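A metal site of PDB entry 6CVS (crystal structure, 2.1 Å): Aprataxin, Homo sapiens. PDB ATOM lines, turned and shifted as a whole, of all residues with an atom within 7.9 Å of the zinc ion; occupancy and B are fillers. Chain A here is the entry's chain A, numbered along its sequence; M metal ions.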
ATOM      1  N   ARG A 158      -0.974   4.600  -1.422  1.00  0.00           N
ATOM      2  CA  ARG A 158      -1.315   4.068  -2.731  1.00  0.00           C
ATOM      3  C   ARG A 158      -2.798   3.700  -2.759  1.00  0.00           C
ATOM      4  O   ARG A 158      -3.293   3.043  -1.841  1.00  0.00           O
ATOM      5  CB  ARG A 158      -0.451   2.847  -3.061  1.00  0.00           C
ATOM      6  CG  ARG A 158      -0.523   2.417  -4.515  1.00  0.00           C
ATOM      7  CD  ARG A 158       0.591   1.438  -4.869  1.00  0.00           C
ATOM      8  NE  ARG A 158       1.919   2.028  -4.738  1.00  0.00           N
ATOM      9  CZ  ARG A 158       2.442   2.904  -5.588  1.00  0.00           C
ATOM     10  NH1 ARG A 158       1.754   3.296  -6.649  1.00  0.00           N
ATOM     11  NH2 ARG A 158       3.663   3.396  -5.384  1.00  0.00           N
ATOM     12  N   CYS A 159      -3.494   4.140  -3.805  1.00  0.00           N
ATOM     13  CA  CYS A 159      -4.903   3.834  -3.945  1.00  0.00           C
ATOM     14  C   CYS A 159      -5.123   2.333  -4.008  1.00  0.00           C
ATOM     15  O   CYS A 159      -4.345   1.604  -4.638  1.00  0.00           O
ATOM     16  CB  CYS A 159      -5.476   4.501  -5.196  1.00  0.00           C
ATOM     17  SG  CYS A 159      -7.244   4.238  -5.435  1.00  0.00           S
ATOM     18  N   HIS A 160      -6.185   1.857  -3.368  1.00  0.00           N
ATOM     19  CA  HIS A 160      -6.489   0.435  -3.361  1.00  0.00           C
ATOM     20  C   HIS A 160      -7.267  -0.020  -4.591  1.00  0.00           C
ATOM     21  O   HIS A 160      -7.355  -1.227  -4.819  1.00  0.00           O
ATOM     22  CB  HIS A 160      -7.283   0.081  -2.091  1.00  0.00           C
ATOM     23  CG  HIS A 160      -8.651   0.678  -2.046  1.00  0.00           C
ATOM     24  ND1 HIS A 160      -8.883   2.035  -2.180  1.00  0.00           N
ATOM     25  CD2 HIS A 160      -9.867   0.116  -1.860  1.00  0.00           C
ATOM     26  CE1 HIS A 160     -10.180   2.275  -2.086  1.00  0.00           C
ATOM     27  NE2 HIS A 160     -10.797   1.119  -1.889  1.00  0.00           N
ATOM     28  N   GLU A 161      -7.802   0.905  -5.391  1.00  0.00           N
ATOM     29  CA  GLU A 161      -8.599   0.576  -6.568  1.00  0.00           C
ATOM     30  C   GLU A 161      -7.780   0.619  -7.853  1.00  0.00           C
ATOM     31  O   GLU A 161      -7.882  -0.295  -8.676  1.00  0.00           O
ATOM     32  CB  GLU A 161      -9.792   1.526  -6.688  1.00  0.00           C
ATOM     33  CG  GLU A 161     -10.727   1.522  -5.482  1.00  0.00           C
ATOM     34  CD  GLU A 161     -11.569   0.263  -5.398  1.00  0.00           C
ATOM     35  OE1 GLU A 161     -11.456  -0.594  -6.299  1.00  0.00           O
ATOM     36  OE2 GLU A 161     -12.341   0.128  -4.426  1.00  0.00           O
ATOM     37  N   CYS A 162      -6.966   1.663  -8.032  1.00  0.00           N
ATOM     38  CA  CYS A 162      -6.156   1.830  -9.236  1.00  0.00           C
ATOM     39  C   CYS A 162      -4.662   1.880  -8.946  1.00  0.00           C
ATOM     40  O   CYS A 162      -3.875   2.042  -9.886  1.00  0.00           O
ATOM     41  CB  CYS A 162      -6.578   3.090  -9.996  1.00  0.00           C
ATOM     42  SG  CYS A 162      -6.109   4.628  -9.181  1.00  0.00           S
ATOM     43  N   GLN A 163      -4.258   1.765  -7.687  1.00  0.00           N
ATOM     44  CA  GLN A 163      -2.848   1.689  -7.301  1.00  0.00           C
ATOM     45  C   GLN A 163      -2.077   2.971  -7.574  1.00  0.00           C
ATOM     46  O   GLN A 163      -0.845   2.973  -7.555  1.00  0.00           O
ATOM     47  CB  GLN A 163      -2.147   0.509  -7.981  1.00  0.00           C
ATOM     48  CG  GLN A 163      -2.556  -0.856  -7.430  1.00  0.00           C
ATOM     49  CD  GLN A 163      -3.911  -1.297  -7.926  1.00  0.00           C
ATOM     50  OE1 GLN A 163      -4.196  -1.245  -9.123  1.00  0.00           O
ATOM     51  NE2 GLN A 163      -4.768  -1.747  -7.005  1.00  0.00           N
ATOM     52  N   GLN A 164      -2.767   4.083  -7.818  1.00  0.00           N
ATOM     53  CA  GLN A 164      -2.075   5.345  -8.022  1.00  0.00           C
ATOM     54  C   GLN A 164      -1.421   5.817  -6.731  1.00  0.00           C
ATOM     55  O   GLN A 164      -2.006   5.714  -5.649  1.00  0.00           O
ATOM     56  CB  GLN A 164      -3.037   6.408  -8.550  1.00  0.00           C
ATOM     57  CG  GLN A 164      -2.414   7.797  -8.657  1.00  0.00           C
ATOM     58  CD  GLN A 164      -3.259   8.765  -9.463  1.00  0.00           C
ATOM     59  OE1 GLN A 164      -4.171   8.356 -10.193  1.00  0.00           O
ATOM     60  NE2 GLN A 164      -2.968  10.051  -9.332  1.00  0.00           N
ATOM     61  N   LEU A 165      -0.201   6.341  -6.851  1.00  0.00           N
ATOM     62  CA  LEU A 165       0.517   6.872  -5.710  1.00  0.00           C
ATOM     63  C   LEU A 165       0.030   8.280  -5.399  1.00  0.00           C
ATOM     64  O   LEU A 165      -0.126   9.110  -6.308  1.00  0.00           O
ATOM     65  CB  LEU A 165       2.022   6.898  -5.988  1.00  0.00           C
ATOM     66  CG  LEU A 165       2.922   7.659  -5.008  1.00  0.00           C
ATOM     67  CD1 LEU A 165       3.085   6.889  -3.705  1.00  0.00           C
ATOM     68  CD2 LEU A 165       4.273   7.943  -5.635  1.00  0.00           C
ATOM     69  N   LEU A 166      -0.237   8.557  -4.122  1.00  0.00           N
ATOM     70  CA  LEU A 166      -0.643   9.881  -3.702  1.00  0.00           C
ATOM     71  C   LEU A 166       0.316  10.430  -2.645  1.00  0.00           C
ATOM     72  O   LEU A 166       0.796   9.677  -1.791  1.00  0.00           O
ATOM     73  CB  LEU A 166      -2.083   9.867  -3.136  1.00  0.00           C
ATOM     74  CG  LEU A 166      -3.241   9.868  -4.149  1.00  0.00           C
ATOM     75  CD1 LEU A 166      -3.115  10.991  -5.168  1.00  0.00           C
ATOM     76  CD2 LEU A 166      -3.384   8.517  -4.840  1.00  0.00           C
ATOM     77  N   LEU A 172      -5.035  11.903  -1.068  1.00  0.00           N
ATOM     78  CA  LEU A 172      -5.600  10.562  -1.190  1.00  0.00           C
ATOM     79  C   LEU A 172      -7.113  10.602  -1.024  1.00  0.00           C
ATOM     80  O   LEU A 172      -7.854  10.060  -1.860  1.00  0.00           O
ATOM     81  CB  LEU A 172      -4.974   9.617  -0.165  1.00  0.00           C
ATOM     82  CG  LEU A 172      -5.529   8.187  -0.207  1.00  0.00           C
ATOM     83  CD1 LEU A 172      -5.152   7.506  -1.521  1.00  0.00           C
ATOM     84  CD2 LEU A 172      -5.025   7.375   0.980  1.00  0.00           C
ATOM     85  N   HIS A 175      -8.677  11.791  -4.043  1.00  0.00           N
ATOM     86  CA  HIS A 175      -8.608  10.832  -5.137  1.00  0.00           C
ATOM     87  C   HIS A 175      -9.657   9.742  -4.977  1.00  0.00           C
ATOM     88  O   HIS A 175     -10.258   9.300  -5.971  1.00  0.00           O
ATOM     89  CB  HIS A 175      -7.206  10.213  -5.200  1.00  0.00           C
ATOM     90  CG  HIS A 175      -7.084   9.086  -6.175  1.00  0.00           C
ATOM     91  ND1 HIS A 175      -6.749   9.266  -7.495  1.00  0.00           N
ATOM     92  CD2 HIS A 175      -7.260   7.746  -6.014  1.00  0.00           C
ATOM     93  CE1 HIS A 175      -6.726   8.095  -8.111  1.00  0.00           C
ATOM     94  NE2 HIS A 175      -7.029   7.160  -7.228  1.00  0.00           N
ATOM     95  N   LEU A 176      -9.890   9.280  -3.749  1.00  0.00           N
ATOM     96  CA  LEU A 176     -10.838   8.182  -3.534  1.00  0.00           C
ATOM     97  C   LEU A 176     -12.239   8.559  -3.991  1.00  0.00           C
ATOM     98  O   LEU A 176     -13.038   7.671  -4.340  1.00  0.00           O
ATOM     99  CB  LEU A 176     -10.850   7.774  -2.056  1.00  0.00           C
ATOM    100  CG  LEU A 176      -9.549   7.171  -1.530  1.00  0.00           C
ATOM    101  CD1 LEU A 176      -9.649   6.886  -0.041  1.00  0.00           C
ATOM    102  CD2 LEU A 176      -9.177   5.896  -2.278  1.00  0.00           C
ATOM    103  N   ARG A 177     -12.584   9.851  -3.991  1.00  0.00           N
ATOM    104  CA  ARG A 177     -13.880  10.273  -4.507  1.00  0.00           C
ATOM    105  C   ARG A 177     -14.114   9.772  -5.926  1.00  0.00           C
ATOM    106  O   ARG A 177     -15.250   9.483  -6.309  1.00  0.00           O
ATOM    107  CB  ARG A 177     -14.006  11.800  -4.467  1.00  0.00           C
ATOM    108  CG  ARG A 177     -13.858  12.410  -3.089  1.00  0.00           C
ATOM    109  CD  ARG A 177     -14.161  13.909  -3.123  1.00  0.00           C
ATOM    110  NE  ARG A 177     -15.380  14.241  -2.388  1.00  0.00           N
ATOM    111  CZ  ARG A 177     -16.599  14.345  -2.922  1.00  0.00           C
ATOM    112  NH1 ARG A 177     -16.787  14.151  -4.227  1.00  0.00           N
ATOM    113  NH2 ARG A 177     -17.632  14.649  -2.157  1.00  0.00           N
ATOM    114  N   LYS A 178     -13.038   9.665  -6.721  1.00  0.00           N
ATOM    115  CA  LYS A 178     -13.178   9.282  -8.117  1.00  0.00           C
ATOM    116  C   LYS A 178     -13.722   7.865  -8.293  1.00  0.00           C
ATOM    117  O   LYS A 178     -14.260   7.558  -9.354  1.00  0.00           O
ATOM    118  CB  LYS A 178     -11.833   9.412  -8.830  1.00  0.00           C
ATOM    119  CG  LYS A 178     -11.328  10.845  -8.958  1.00  0.00           C
ATOM    120  CD  LYS A 178      -9.923  10.890  -9.526  1.00  0.00           C
ATOM    121  CE  LYS A 178      -9.611  12.239 -10.165  1.00  0.00           C
ATOM    122  NZ  LYS A 178      -8.184  12.333 -10.605  1.00  0.00           N
ATOM    123  N   HIS A 179     -13.593   7.010  -7.280  1.00  0.00           N
ATOM    124  CA  HIS A 179     -13.980   5.614  -7.390  1.00  0.00           C
ATOM    125  C   HIS A 179     -15.350   5.325  -6.800  1.00  0.00           C
ATOM    126  O   HIS A 179     -15.711   4.153  -6.636  1.00  0.00           O
ATOM    127  CB  HIS A 179     -12.923   4.726  -6.732  1.00  0.00           C
ATOM    128  CG  HIS A 179     -11.575   4.826  -7.384  1.00  0.00           C
ATOM    129  ND1 HIS A 179     -11.360   4.497  -8.704  1.00  0.00           N
ATOM    130  CD2 HIS A 179     -10.384   5.215  -6.895  1.00  0.00           C
ATOM    131  CE1 HIS A 179     -10.089   4.680  -9.002  1.00  0.00           C
ATOM    132  NE2 HIS A 179      -9.468   5.118  -7.915  1.00  0.00           N
HETATM  133 ZN    ZN M   1      -7.528   5.218  -7.522  1.00  0.00          ZN
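The zinc ion is bound by a ring nitrogen (NE2) of His 179 (2.0 Å), a ring nitrogen (NE2) of His 175 (2.0 Å), the side-chain sulfur (SG) of Cys 162 (2.3 Å) and the side-chain sulfur (SG) of Cys 159 (2.3 Å).
The side-chain sulfur of Cys 159 lies close to the backbone NH of Glu 161 (3.4 Å).
N of Gln 164 sits close to SG of Cys 162 (3.7 Å).
The backbone NH (N) of Cys 159 lies within hydrogen-bond range of the backbone carbonyl oxygen (O) of Gln 164, 2.8 Å away.
The nearest printed residue that does not touch the zinc ion is Glu 161 (4.4 Å).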
